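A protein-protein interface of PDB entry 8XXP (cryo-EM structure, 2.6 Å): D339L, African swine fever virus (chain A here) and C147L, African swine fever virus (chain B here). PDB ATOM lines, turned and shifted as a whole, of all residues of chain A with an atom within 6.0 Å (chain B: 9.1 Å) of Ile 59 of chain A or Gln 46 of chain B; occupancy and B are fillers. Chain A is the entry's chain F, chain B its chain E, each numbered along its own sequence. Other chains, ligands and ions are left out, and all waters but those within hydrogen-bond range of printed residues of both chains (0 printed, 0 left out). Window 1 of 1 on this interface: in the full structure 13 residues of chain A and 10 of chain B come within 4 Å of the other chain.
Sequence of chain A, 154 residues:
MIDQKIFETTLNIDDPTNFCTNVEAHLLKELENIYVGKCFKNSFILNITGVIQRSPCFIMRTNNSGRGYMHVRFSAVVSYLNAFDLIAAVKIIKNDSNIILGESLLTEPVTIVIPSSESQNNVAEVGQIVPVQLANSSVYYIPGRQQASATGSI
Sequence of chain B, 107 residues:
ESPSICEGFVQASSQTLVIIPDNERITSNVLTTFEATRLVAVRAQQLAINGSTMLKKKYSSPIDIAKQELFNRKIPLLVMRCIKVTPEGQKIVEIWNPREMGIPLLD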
ATOM      1  N   ASP A  15     -19.382  14.429 -11.192  1.00  0.00           N
ATOM      2  CA  ASP A  15     -18.580  14.098 -12.368  1.00  0.00           C
ATOM      3  C   ASP A  15     -17.454  15.115 -12.447  1.00  0.00           C
ATOM      4  O   ASP A  15     -17.525  16.080 -13.218  1.00  0.00           O
ATOM      5  CB  ASP A  15     -19.428  14.092 -13.640  1.00  0.00           C
ATOM      6  CG  ASP A  15     -18.771  13.335 -14.779  1.00  0.00           C
ATOM      7  OD1 ASP A  15     -17.527  13.322 -14.852  1.00  0.00           O
ATOM      8  OD2 ASP A  15     -19.501  12.749 -15.601  1.00  0.00           O
ATOM      9  N   PRO A  16     -16.405  14.942 -11.640  1.00  0.00           N
ATOM     10  CA  PRO A  16     -15.317  15.934 -11.621  1.00  0.00           C
ATOM     11  C   PRO A  16     -14.532  16.020 -12.914  1.00  0.00           C
ATOM     12  O   PRO A  16     -13.911  17.057 -13.171  1.00  0.00           O
ATOM     13  CB  PRO A  16     -14.439  15.467 -10.455  1.00  0.00           C
ATOM     14  CG  PRO A  16     -14.775  14.047 -10.270  1.00  0.00           C
ATOM     15  CD  PRO A  16     -16.195  13.874 -10.654  1.00  0.00           C
ATOM     16  N   THR A  17     -14.527  14.971 -13.735  1.00  0.00           N
ATOM     17  CA  THR A  17     -13.844  15.053 -15.021  1.00  0.00           C
ATOM     18  C   THR A  17     -14.620  15.931 -15.993  1.00  0.00           C
ATOM     19  O   THR A  17     -14.039  16.772 -16.686  1.00  0.00           O
ATOM     20  CB  THR A  17     -13.648  13.656 -15.604  1.00  0.00           C
ATOM     21  OG1 THR A  17     -13.335  12.738 -14.550  1.00  0.00           O
ATOM     22  CG2 THR A  17     -12.520  13.664 -16.623  1.00  0.00           C
ATOM     23  N   CYS A  57     -10.947  21.938  -7.573  1.00  0.00           N
ATOM     24  CA  CYS A  57     -11.855  20.804  -7.441  1.00  0.00           C
ATOM     25  C   CYS A  57     -11.160  19.733  -6.610  1.00  0.00           C
ATOM     26  O   CYS A  57     -10.572  18.779  -7.120  1.00  0.00           O
ATOM     27  CB  CYS A  57     -12.265  20.268  -8.805  1.00  0.00           C
ATOM     28  SG  CYS A  57     -13.459  18.921  -8.730  1.00  0.00           S
ATOM     29  N   PHE A  58     -11.218  19.912  -5.295  1.00  0.00           N
ATOM     30  CA  PHE A  58     -10.701  18.902  -4.390  1.00  0.00           C
ATOM     31  C   PHE A  58     -11.483  17.613  -4.568  1.00  0.00           C
ATOM     32  O   PHE A  58     -12.685  17.638  -4.812  1.00  0.00           O
ATOM     33  CB  PHE A  58     -10.815  19.368  -2.942  1.00  0.00           C
ATOM     34  CG  PHE A  58     -10.187  20.698  -2.668  1.00  0.00           C
ATOM     35  CD1 PHE A  58      -8.819  20.847  -2.684  1.00  0.00           C
ATOM     36  CD2 PHE A  58     -10.967  21.791  -2.359  1.00  0.00           C
ATOM     37  CE1 PHE A  58      -8.242  22.065  -2.423  1.00  0.00           C
ATOM     38  CE2 PHE A  58     -10.391  23.008  -2.089  1.00  0.00           C
ATOM     39  CZ  PHE A  58      -9.027  23.144  -2.123  1.00  0.00           C
ATOM     40  N   ILE A  59     -10.800  16.487  -4.450  1.00  0.00           N
ATOM     41  CA  ILE A  59     -11.451  15.184  -4.471  1.00  0.00           C
ATOM     42  C   ILE A  59     -11.832  14.826  -3.046  1.00  0.00           C
ATOM     43  O   ILE A  59     -11.036  15.020  -2.121  1.00  0.00           O
ATOM     44  CB  ILE A  59     -10.531  14.118  -5.088  1.00  0.00           C
ATOM     45  CG1 ILE A  59     -10.225  14.462  -6.544  1.00  0.00           C
ATOM     46  CG2 ILE A  59     -11.166  12.744  -5.001  1.00  0.00           C
ATOM     47  CD1 ILE A  59     -11.440  14.776  -7.349  1.00  0.00           C
ATOM     48  N   MET A  60     -13.054  14.332  -2.858  1.00  0.00           N
ATOM     49  CA  MET A  60     -13.503  13.948  -1.528  1.00  0.00           C
ATOM     50  C   MET A  60     -12.569  12.904  -0.946  1.00  0.00           C
ATOM     51  O   MET A  60     -12.194  11.943  -1.618  1.00  0.00           O
ATOM     52  CB  MET A  60     -14.928  13.409  -1.573  1.00  0.00           C
ATOM     53  CG  MET A  60     -15.925  14.378  -2.146  1.00  0.00           C
ATOM     54  SD  MET A  60     -17.592  13.724  -2.179  1.00  0.00           S
ATOM     55  CE  MET A  60     -18.502  15.224  -2.484  1.00  0.00           C
ATOM     56  N   ARG A  61     -12.187  13.102   0.308  1.00  0.00           N
ATOM     57  CA  ARG A  61     -11.193  12.263   0.954  1.00  0.00           C
ATOM     58  C   ARG A  61     -11.798  11.176   1.824  1.00  0.00           C
ATOM     59  O   ARG A  61     -11.235  10.084   1.904  1.00  0.00           O
ATOM     60  CB  ARG A  61     -10.261  13.129   1.802  1.00  0.00           C
ATOM     61  CG  ARG A  61      -9.032  12.427   2.297  1.00  0.00           C
ATOM     62  CD  ARG A  61      -8.262  13.307   3.253  1.00  0.00           C
ATOM     63  NE  ARG A  61      -9.031  13.620   4.450  1.00  0.00           N
ATOM     64  CZ  ARG A  61      -9.193  12.799   5.477  1.00  0.00           C
ATOM     65  NH1 ARG A  61      -8.667  11.587   5.482  1.00  0.00           N
ATOM     66  NH2 ARG A  61      -9.899  13.205   6.527  1.00  0.00           N
ATOM     67  N   SER A  65     -15.952   7.466  -3.183  1.00  0.00           N
ATOM     68  CA  SER A  65     -16.819   7.776  -4.311  1.00  0.00           C
ATOM     69  C   SER A  65     -16.094   8.456  -5.462  1.00  0.00           C
ATOM     70  O   SER A  65     -16.624   8.484  -6.575  1.00  0.00           O
ATOM     71  CB  SER A  65     -17.971   8.657  -3.840  1.00  0.00           C
ATOM     72  OG  SER A  65     -17.489   9.884  -3.338  1.00  0.00           O
ATOM     73  N   GLY A  66     -14.913   9.014  -5.225  1.00  0.00           N
ATOM     74  CA  GLY A  66     -14.206   9.701  -6.281  1.00  0.00           C
ATOM     75  C   GLY A  66     -14.772  11.047  -6.657  1.00  0.00           C
ATOM     76  O   GLY A  66     -14.350  11.617  -7.664  1.00  0.00           O
ATOM     77  N   ARG A  67     -15.713  11.574  -5.883  1.00  0.00           N
ATOM     78  CA  ARG A  67     -16.336  12.845  -6.203  1.00  0.00           C
ATOM     79  C   ARG A  67     -15.489  14.007  -5.693  1.00  0.00           C
ATOM     80  O   ARG A  67     -14.545  13.837  -4.921  1.00  0.00           O
ATOM     81  CB  ARG A  67     -17.742  12.913  -5.616  1.00  0.00           C
ATOM     82  CG  ARG A  67     -18.739  12.018  -6.305  1.00  0.00           C
ATOM     83  CD  ARG A  67     -19.772  11.492  -5.338  1.00  0.00           C
ATOM     84  NE  ARG A  67     -20.587  12.547  -4.749  1.00  0.00           N
ATOM     85  CZ  ARG A  67     -21.062  12.518  -3.510  1.00  0.00           C
ATOM     86  NH1 ARG A  67     -20.792  11.518  -2.690  1.00  0.00           N
ATOM     87  NH2 ARG A  67     -21.829  13.518  -3.088  1.00  0.00           N
ATOM     88  N   GLY A  68     -15.838  15.204  -6.145  1.00  0.00           N
ATOM     89  CA  GLY A  68     -15.151  16.405  -5.721  1.00  0.00           C
ATOM     90  C   GLY A  68     -16.110  17.400  -5.119  1.00  0.00           C
ATOM     91  O   GLY A  68     -17.319  17.225  -5.261  1.00  0.00           O
ATOM     92  N   TYR A  69     -15.626  18.431  -4.426  1.00  0.00           N
ATOM     93  CA  TYR A  69     -16.559  19.382  -3.835  1.00  0.00           C
ATOM     94  C   TYR A  69     -16.421  20.805  -4.361  1.00  0.00           C
ATOM     95  O   TYR A  69     -17.411  21.342  -4.862  1.00  0.00           O
ATOM     96  CB  TYR A  69     -16.499  19.343  -2.299  1.00  0.00           C
ATOM     97  CG  TYR A  69     -15.161  19.183  -1.620  1.00  0.00           C
ATOM     98  CD1 TYR A  69     -14.484  17.976  -1.651  1.00  0.00           C
ATOM     99  CD2 TYR A  69     -14.615  20.216  -0.876  1.00  0.00           C
ATOM    100  CE1 TYR A  69     -13.288  17.821  -1.007  1.00  0.00           C
ATOM    101  CE2 TYR A  69     -13.421  20.066  -0.233  1.00  0.00           C
ATOM    102  CZ  TYR A  69     -12.761  18.868  -0.297  1.00  0.00           C
ATOM    103  OH  TYR A  69     -11.563  18.712   0.347  1.00  0.00           O
ATOM    104  N   ARG B  38      -2.966   6.684  -4.393  1.00  0.00           N
ATOM    105  CA  ARG B  38      -4.154   7.521  -4.310  1.00  0.00           C
ATOM    106  C   ARG B  38      -4.524   8.095  -5.669  1.00  0.00           C
ATOM    107  O   ARG B  38      -5.707   8.180  -6.010  1.00  0.00           O
ATOM    108  CB  ARG B  38      -3.924   8.637  -3.295  1.00  0.00           C
ATOM    109  CG  ARG B  38      -5.018   9.675  -3.237  1.00  0.00           C
ATOM    110  CD  ARG B  38      -6.307   9.111  -2.697  1.00  0.00           C
ATOM    111  NE  ARG B  38      -7.277  10.167  -2.456  1.00  0.00           N
ATOM    112  CZ  ARG B  38      -8.567   9.966  -2.237  1.00  0.00           C
ATOM    113  NH1 ARG B  38      -9.083   8.751  -2.223  1.00  0.00           N
ATOM    114  NH2 ARG B  38      -9.358  11.010  -2.018  1.00  0.00           N
ATOM    115  N   LEU B  39      -3.530   8.509  -6.456  1.00  0.00           N
ATOM    116  CA  LEU B  39      -3.810   9.040  -7.783  1.00  0.00           C
ATOM    117  C   LEU B  39      -4.447   7.986  -8.669  1.00  0.00           C
ATOM    118  O   LEU B  39      -5.432   8.255  -9.365  1.00  0.00           O
ATOM    119  CB  LEU B  39      -2.526   9.554  -8.425  1.00  0.00           C
ATOM    120  CG  LEU B  39      -1.973  10.873  -7.914  1.00  0.00           C
ATOM    121  CD1 LEU B  39      -0.569  11.033  -8.419  1.00  0.00           C
ATOM    122  CD2 LEU B  39      -2.842  12.021  -8.363  1.00  0.00           C
ATOM    123  N   VAL B  40      -3.899   6.772  -8.651  1.00  0.00           N
ATOM    124  CA  VAL B  40      -4.467   5.704  -9.463  1.00  0.00           C
ATOM    125  C   VAL B  40      -5.871   5.361  -8.988  1.00  0.00           C
ATOM    126  O   VAL B  40      -6.772   5.145  -9.800  1.00  0.00           O
ATOM    127  CB  VAL B  40      -3.542   4.475  -9.465  1.00  0.00           C
ATOM    128  CG1 VAL B  40      -4.153   3.353 -10.269  1.00  0.00           C
ATOM    129  CG2 VAL B  40      -2.205   4.839 -10.053  1.00  0.00           C
ATOM    130  N   ALA B  41      -6.088   5.319  -7.672  1.00  0.00           N
ATOM    131  CA  ALA B  41      -7.407   4.981  -7.147  1.00  0.00           C
ATOM    132  C   ALA B  41      -8.445   6.029  -7.519  1.00  0.00           C
ATOM    133  O   ALA B  41      -9.560   5.690  -7.929  1.00  0.00           O
ATOM    134  CB  ALA B  41      -7.339   4.815  -5.633  1.00  0.00           C
ATOM    135  N   VAL B  42      -8.097   7.308  -7.386  1.00  0.00           N
ATOM    136  CA  VAL B  42      -9.020   8.377  -7.752  1.00  0.00           C
ATOM    137  C   VAL B  42      -9.321   8.330  -9.242  1.00  0.00           C
ATOM    138  O   VAL B  42     -10.480   8.428  -9.664  1.00  0.00           O
ATOM    139  CB  VAL B  42      -8.450   9.743  -7.335  1.00  0.00           C
ATOM    140  CG1 VAL B  42      -9.258  10.863  -7.947  1.00  0.00           C
ATOM    141  CG2 VAL B  42      -8.444   9.866  -5.838  1.00  0.00           C
ATOM    142  N   ARG B  43      -8.282   8.172 -10.065  1.00  0.00           N
ATOM    143  CA  ARG B  43      -8.495   8.147 -11.504  1.00  0.00           C
ATOM    144  C   ARG B  43      -9.344   6.956 -11.915  1.00  0.00           C
ATOM    145  O   ARG B  43     -10.207   7.073 -12.789  1.00  0.00           O
ATOM    146  CB  ARG B  43      -7.156   8.123 -12.233  1.00  0.00           C
ATOM    147  CG  ARG B  43      -7.294   8.233 -13.730  1.00  0.00           C
ATOM    148  CD  ARG B  43      -8.036   9.491 -14.102  1.00  0.00           C
ATOM    149  NE  ARG B  43      -8.296   9.573 -15.534  1.00  0.00           N
ATOM    150  CZ  ARG B  43      -9.323  10.222 -16.066  1.00  0.00           C
ATOM    151  NH1 ARG B  43     -10.205  10.856 -15.313  1.00  0.00           N
ATOM    152  NH2 ARG B  43      -9.464  10.240 -17.386  1.00  0.00           N
ATOM    153  N   ALA B  44      -9.126   5.801 -11.286  1.00  0.00           N
ATOM    154  CA  ALA B  44      -9.875   4.608 -11.643  1.00  0.00           C
ATOM    155  C   ALA B  44     -11.326   4.705 -11.195  1.00  0.00           C
ATOM    156  O   ALA B  44     -12.229   4.250 -11.902  1.00  0.00           O
ATOM    157  CB  ALA B  44      -9.195   3.380 -11.048  1.00  0.00           C
ATOM    158  N   GLN B  45     -11.582   5.306 -10.033  1.00  0.00           N
ATOM    159  CA  GLN B  45     -12.968   5.520  -9.630  1.00  0.00           C
ATOM    160  C   GLN B  45     -13.671   6.493 -10.570  1.00  0.00           C
ATOM    161  O   GLN B  45     -14.837   6.288 -10.935  1.00  0.00           O
ATOM    162  CB  GLN B  45     -13.026   6.018  -8.189  1.00  0.00           C
ATOM    163  CG  GLN B  45     -14.430   6.173  -7.650  1.00  0.00           C
ATOM    164  CD  GLN B  45     -15.186   4.868  -7.615  1.00  0.00           C
ATOM    165  OE1 GLN B  45     -14.612   3.815  -7.367  1.00  0.00           O
ATOM    166  NE2 GLN B  45     -16.482   4.931  -7.871  1.00  0.00           N
ATOM    167  N   GLN B  46     -12.980   7.553 -10.978  1.00  0.00           N
ATOM    168  CA  GLN B  46     -13.589   8.494 -11.909  1.00  0.00           C
ATOM    169  C   GLN B  46     -13.775   7.880 -13.288  1.00  0.00           C
ATOM    170  O   GLN B  46     -14.676   8.286 -14.026  1.00  0.00           O
ATOM    171  CB  GLN B  46     -12.751   9.761 -11.986  1.00  0.00           C
ATOM    172  CG  GLN B  46     -12.815  10.588 -10.725  1.00  0.00           C
ATOM    173  CD  GLN B  46     -11.782  11.676 -10.710  1.00  0.00           C
ATOM    174  OE1 GLN B  46     -10.898  11.712 -11.558  1.00  0.00           O
ATOM    175  NE2 GLN B  46     -11.887  12.576  -9.749  1.00  0.00           N
ATOM    176  N   LEU B  47     -12.936   6.915 -13.658  1.00  0.00           N
ATOM    177  CA  LEU B  47     -13.165   6.146 -14.872  1.00  0.00           C
ATOM    178  C   LEU B  47     -14.266   5.117 -14.697  1.00  0.00           C
ATOM    179  O   LEU B  47     -14.753   4.566 -15.686  1.00  0.00           O
ATOM    180  CB  LEU B  47     -11.888   5.437 -15.305  1.00  0.00           C
ATOM    181  CG  LEU B  47     -10.829   6.350 -15.900  1.00  0.00           C
ATOM    182  CD1 LEU B  47      -9.466   5.719 -15.734  1.00  0.00           C
ATOM    183  CD2 LEU B  47     -11.144   6.638 -17.344  1.00  0.00           C
ATOM    184  N   ALA B  48     -14.617   4.796 -13.458  1.00  0.00           N
ATOM    185  CA  ALA B  48     -15.807   3.997 -13.223  1.00  0.00           C
ATOM    186  C   ALA B  48     -17.066   4.842 -13.358  1.00  0.00           C
ATOM    187  O   ALA B  48     -18.108   4.340 -13.786  1.00  0.00           O
ATOM    188  CB  ALA B  48     -15.736   3.336 -11.848  1.00  0.00           C
ATOM    189  N   ILE B  49     -16.997   6.121 -13.006  1.00  0.00           N
ATOM    190  CA  ILE B  49     -18.177   6.970 -13.161  1.00  0.00           C
ATOM    191  C   ILE B  49     -18.242   7.595 -14.554  1.00  0.00           C
ATOM    192  O   ILE B  49     -19.320   7.686 -15.143  1.00  0.00           O
ATOM    193  CB  ILE B  49     -18.238   8.036 -12.043  1.00  0.00           C
ATOM    194  CG1 ILE B  49     -17.227   9.162 -12.262  1.00  0.00           C
ATOM    195  CG2 ILE B  49     -18.018   7.384 -10.684  1.00  0.00           C
ATOM    196  CD1 ILE B  49     -17.028  10.046 -11.049  1.00  0.00           C
ATOM    197  N   ASN B  50     -17.117   8.039 -15.103  1.00  0.00           N
ATOM    198  CA  ASN B  50     -17.025   8.540 -16.462  1.00  0.00           C
ATOM    199  C   ASN B  50     -16.366   7.479 -17.335  1.00  0.00           C
ATOM    200  O   ASN B  50     -16.208   6.327 -16.931  1.00  0.00           O
ATOM    201  CB  ASN B  50     -16.262   9.862 -16.495  1.00  0.00           C
ATOM    202  CG  ASN B  50     -16.907  10.879 -17.407  1.00  0.00           C
ATOM    203  OD1 ASN B  50     -18.091  10.780 -17.722  1.00  0.00           O
ATOM    204  ND2 ASN B  50     -16.131  11.863 -17.839  1.00  0.00           N
ATOM    205  N   GLY B  51     -16.009   7.843 -18.561  1.00  0.00           N
ATOM    206  CA  GLY B  51     -15.309   6.895 -19.405  1.00  0.00           C
ATOM    207  C   GLY B  51     -14.262   7.483 -20.328  1.00  0.00           C
ATOM    208  O   GLY B  51     -13.698   6.762 -21.155  1.00  0.00           O
ATOM    209  N   SER B  52     -13.974   8.773 -20.197  1.00  0.00           N
ATOM    210  CA  SER B  52     -13.120   9.466 -21.152  1.00  0.00           C
ATOM    211  C   SER B  52     -11.661   9.345 -20.742  1.00  0.00           C
ATOM    212  O   SER B  52     -11.293   9.698 -19.619  1.00  0.00           O
ATOM    213  CB  SER B  52     -13.514  10.939 -21.261  1.00  0.00           C
ATOM    214  OG  SER B  52     -13.466  11.575 -19.998  1.00  0.00           O
ATOM    215  N   THR B  53     -10.830   8.864 -21.666  1.00  0.00           N
ATOM    216  CA  THR B  53      -9.415   8.648 -21.404  1.00  0.00           C
ATOM    217  C   THR B  53      -8.601   9.258 -22.536  1.00  0.00           C
ATOM    218  O   THR B  53      -9.104   9.484 -23.638  1.00  0.00           O
ATOM    219  CB  THR B  53      -9.057   7.158 -21.286  1.00  0.00           C
ATOM    220  OG1 THR B  53      -8.741   6.644 -22.581  1.00  0.00           O
ATOM    221  CG2 THR B  53     -10.217   6.362 -20.751  1.00  0.00           C
ATOM    222  N   PRO B  62     -10.967  -0.096 -15.418  1.00  0.00           N
ATOM    223  CA  PRO B  62     -10.564   1.268 -15.049  1.00  0.00           C
ATOM    224  C   PRO B  62      -9.240   1.313 -14.321  1.00  0.00           C
ATOM    225  O   PRO B  62      -8.509   2.300 -14.439  1.00  0.00           O
ATOM    226  CB  PRO B  62     -11.716   1.741 -14.156  1.00  0.00           C
ATOM    227  CG  PRO B  62     -12.296   0.500 -13.607  1.00  0.00           C
ATOM    228  CD  PRO B  62     -12.154  -0.542 -14.672  1.00  0.00           C
ATOM    229  N   ILE B  63      -8.918   0.265 -13.560  1.00  0.00           N
ATOM    230  CA  ILE B  63      -7.654   0.219 -12.835  1.00  0.00           C
ATOM    231  C   ILE B  63      -6.484   0.187 -13.806  1.00  0.00           C
ATOM    232  O   ILE B  63      -5.476   0.872 -13.606  1.00  0.00           O
ATOM    233  CB  ILE B  63      -7.636  -0.986 -11.881  1.00  0.00           C
ATOM    234  CG1 ILE B  63      -8.809  -0.898 -10.903  1.00  0.00           C
ATOM    235  CG2 ILE B  63      -6.315  -1.061 -11.143  1.00  0.00           C
ATOM    236  CD1 ILE B  63      -8.790  -1.931  -9.825  1.00  0.00           C
ATOM    237  N   ILE B  65      -6.505   1.301 -16.921  1.00  0.00           N
ATOM    238  CA  ILE B  65      -6.445   2.604 -17.573  1.00  0.00           C
ATOM    239  C   ILE B  65      -5.747   3.615 -16.675  1.00  0.00           C
ATOM    240  O   ILE B  65      -4.889   4.380 -17.125  1.00  0.00           O
ATOM    241  CB  ILE B  65      -7.856   3.077 -17.967  1.00  0.00           C
ATOM    242  CG1 ILE B  65      -8.531   2.059 -18.879  1.00  0.00           C
ATOM    243  CG2 ILE B  65      -7.791   4.421 -18.649  1.00  0.00           C
ATOM    244  CD1 ILE B  65     -10.011   2.273 -19.040  1.00  0.00           C
ATOM    245  N   ALA B  66      -6.102   3.634 -15.388  1.00  0.00           N
ATOM    246  CA  ALA B  66      -5.487   4.582 -14.464  1.00  0.00           C
ATOM    247  C   ALA B  66      -4.005   4.294 -14.267  1.00  0.00           C
ATOM    248  O   ALA B  66      -3.189   5.221 -14.199  1.00  0.00           O
ATOM    249  CB  ALA B  66      -6.223   4.561 -13.128  1.00  0.00           C
ATOM    250  N   GLU B  69      -2.236   5.467 -17.324  1.00  0.00           N
ATOM    251  CA  GLU B  69      -2.229   6.923 -17.377  1.00  0.00           C
ATOM    252  C   GLU B  69      -1.165   7.496 -16.456  1.00  0.00           C
ATOM    253  O   GLU B  69      -0.477   8.456 -16.811  1.00  0.00           O
ATOM    254  CB  GLU B  69      -3.605   7.470 -17.013  1.00  0.00           C
ATOM    255  CG  GLU B  69      -4.354   8.068 -18.181  1.00  0.00           C
ATOM    256  CD  GLU B  69      -5.813   8.303 -17.874  1.00  0.00           C
ATOM    257  OE1 GLU B  69      -6.148   8.491 -16.688  1.00  0.00           O
ATOM    258  OE2 GLU B  69      -6.629   8.311 -18.817  1.00  0.00           O
ATOM    259  N   ILE B  75      -2.237  11.466 -16.614  1.00  0.00           N
ATOM    260  CA  ILE B  75      -3.288  11.423 -15.597  1.00  0.00           C
ATOM    261  C   ILE B  75      -3.748  12.851 -15.304  1.00  0.00           C
ATOM    262  O   ILE B  75      -2.907  13.728 -15.060  1.00  0.00           O
ATOM    263  CB  ILE B  75      -2.784  10.716 -14.339  1.00  0.00           C
ATOM    264  CG1 ILE B  75      -3.908  10.497 -13.333  1.00  0.00           C
ATOM    265  CG2 ILE B  75      -1.587  11.433 -13.722  1.00  0.00           C
ATOM    266  CD1 ILE B  75      -3.692   9.276 -12.479  1.00  0.00           C
ATOM    267  N   PRO B  76      -5.057  13.144 -15.379  1.00  0.00           N
ATOM    268  CA  PRO B  76      -5.542  14.527 -15.299  1.00  0.00           C
ATOM    269  C   PRO B  76      -5.744  15.020 -13.871  1.00  0.00           C
ATOM    270  O   PRO B  76      -6.728  15.693 -13.556  1.00  0.00           O
ATOM    271  CB  PRO B  76      -6.872  14.457 -16.053  1.00  0.00           C
ATOM    272  CG  PRO B  76      -7.366  13.099 -15.725  1.00  0.00           C
ATOM    273  CD  PRO B  76      -6.158  12.203 -15.641  1.00  0.00           C
ATOM    274  N   LEU B  77      -4.791  14.718 -13.000  1.00  0.00           N
ATOM    275  CA  LEU B  77      -4.904  15.042 -11.590  1.00  0.00           C
ATOM    276  C   LEU B  77      -3.678  15.826 -11.161  1.00  0.00           C
ATOM    277  O   LEU B  77      -2.661  15.856 -11.853  1.00  0.00           O
ATOM    278  CB  LEU B  77      -5.054  13.777 -10.734  1.00  0.00           C
ATOM    279  CG  LEU B  77      -6.235  12.861 -11.058  1.00  0.00           C
ATOM    280  CD1 LEU B  77      -6.222  11.633 -10.177  1.00  0.00           C
ATOM    281  CD2 LEU B  77      -7.537  13.605 -10.903  1.00  0.00           C
ATOM    282  N   LEU B  78      -3.795  16.478 -10.012  1.00  0.00           N
ATOM    283  CA  LEU B  78      -2.682  17.175  -9.394  1.00  0.00           C
ATOM    284  C   LEU B  78      -2.584  16.751  -7.940  1.00  0.00           C
ATOM    285  O   LEU B  78      -3.581  16.384  -7.318  1.00  0.00           O
ATOM    286  CB  LEU B  78      -2.844  18.688  -9.474  1.00  0.00           C
ATOM    287  CG  LEU B  78      -2.825  19.324 -10.856  1.00  0.00           C
ATOM    288  CD1 LEU B  78      -3.235  20.764 -10.746  1.00  0.00           C
ATOM    289  CD2 LEU B  78      -1.452  19.199 -11.466  1.00  0.00           C
ATOM    290  N   MET B  80      -1.775  18.135  -4.367  1.00  0.00           N
ATOM    291  CA  MET B  80      -1.627  19.331  -3.554  1.00  0.00           C
ATOM    292  C   MET B  80      -1.146  18.909  -2.174  1.00  0.00           C
ATOM    293  O   MET B  80      -1.825  18.143  -1.485  1.00  0.00           O
ATOM    294  CB  MET B  80      -2.941  20.104  -3.466  1.00  0.00           C
ATOM    295  CG  MET B  80      -3.097  20.898  -2.198  1.00  0.00           C
ATOM    296  SD  MET B  80      -4.572  21.917  -2.197  1.00  0.00           S
ATOM    297  CE  MET B  80      -5.276  21.425  -0.632  1.00  0.00           C
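Cys 57 of chain A touches none of the printed residues of chain B.
Of the printed residues of chain B, Ile 59 of chain A touches Arg 38, Val 42 and Gln 46.
Printed residues of chain B within 4 Å of Ser 65 of chain A: Gln 45.
Of the printed residues of chain A, Val 42 of chain B touches Ile 59.
Of the printed residues of chain A, Arg 43 of chain B touches Thr 17 (3.7 Å).
Of chain A, only Pro 16, Thr 17, Ile 59 and Gly 66 come within 4 Å of Gln 46 of chain B.
Ala 48 of chain B touches none of the printed residues of chain A.
Printed residues of chain A within 4 Å of Asn 50 of chain B: Asp 15 and Thr 17.
Of the printed residues of chain A, Met 80 of chain B touches Phe 58.
The nearest printed residue of chain B that does not touch Thr 17 of chain A is Ser 52 of chain B (4.1 Å).
Hydrophobic or aromatic side chains of chain A within 4 Å of the printed part of chain B: Pro 16, Phe 58 and Ile 59.
Among the printed residues, no Asp or Glu carboxylate lies within 4 Å of a Lys or Arg side-chain nitrogen of the other chain.
The guanidinium group (NH2) of Arg 43 of chain B is in hydrogen-bond range of the backbone carbonyl oxygen (O) of Ser 52 of chain B, 2.9 Å away.
The guanidinium group (NE) of Arg 43 of chain B lies within salt-bridge range of the side-chain carboxylate (OE1) of Glu 69 of chain B, 2.7 Å away.
The side-chain amide nitrogen (ND2) of Asn 50 of chain B sits at hydrogen-bond distance from the side-chain hydroxyl (OG) of Ser 52 of chain B.
The backbone NH (N) of Tyr 69 of chain A sits at hydrogen-bond distance from the backbone carbonyl oxygen (O) of Phe 58 of chain A.
N of Met 60 of chain A lies within hydrogen-bond range of O of Arg 67 of chain A (2.6 Å).
The guanidinium group (NH2) of Arg 38 of chain B is in hydrogen-bond range of the backbone carbonyl oxygen (O) of Met 60 of chain A, at 3.0 Å.
The backbone carbonyl oxygen (O) of Gly 66 of chain A is in hydrogen-bond range of the side-chain amide nitrogen (NE2) of Gln 46 of chain B, at 3.4 Å.
The side-chain amide oxygen (OD1) of Asn 50 of chain B lies close to the side-chain carboxylate (OD2) of Asp 15 of chain A.
Among the printed residues, merely in contact across the chains: Pro 16 of chain A with Gln 46 of chain B (3.3 Å), Pro 16 of chain A with Ile 49 of chain B (3.9 Å), Thr 17 of chain A with Arg 43 of chain B (3.7 Å), Thr 17 of chain A with Gln 46 of chain B (3.97 Å), Thr 17 of chain A with Asn 50 of chain B (3.8 Å), Phe 58 of chain A with Met 80 of chain B (3.5 Å), Ile 59 of chain A with Arg 38 of chain B (3.9 Å), Ile 59 of chain A with Val 42 of chain B (3.98 Å), Ile 59 of chain A with Gln 46 of chain B (3.3 Å), Arg 61 of chain A with Arg 38 of chain B (3.7 Å), Ser 65 of chain A with Gln 45 of chain B (3.4 Å) and Gly 66 of chain A with Gln 45 of chain B (3.8 Å).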
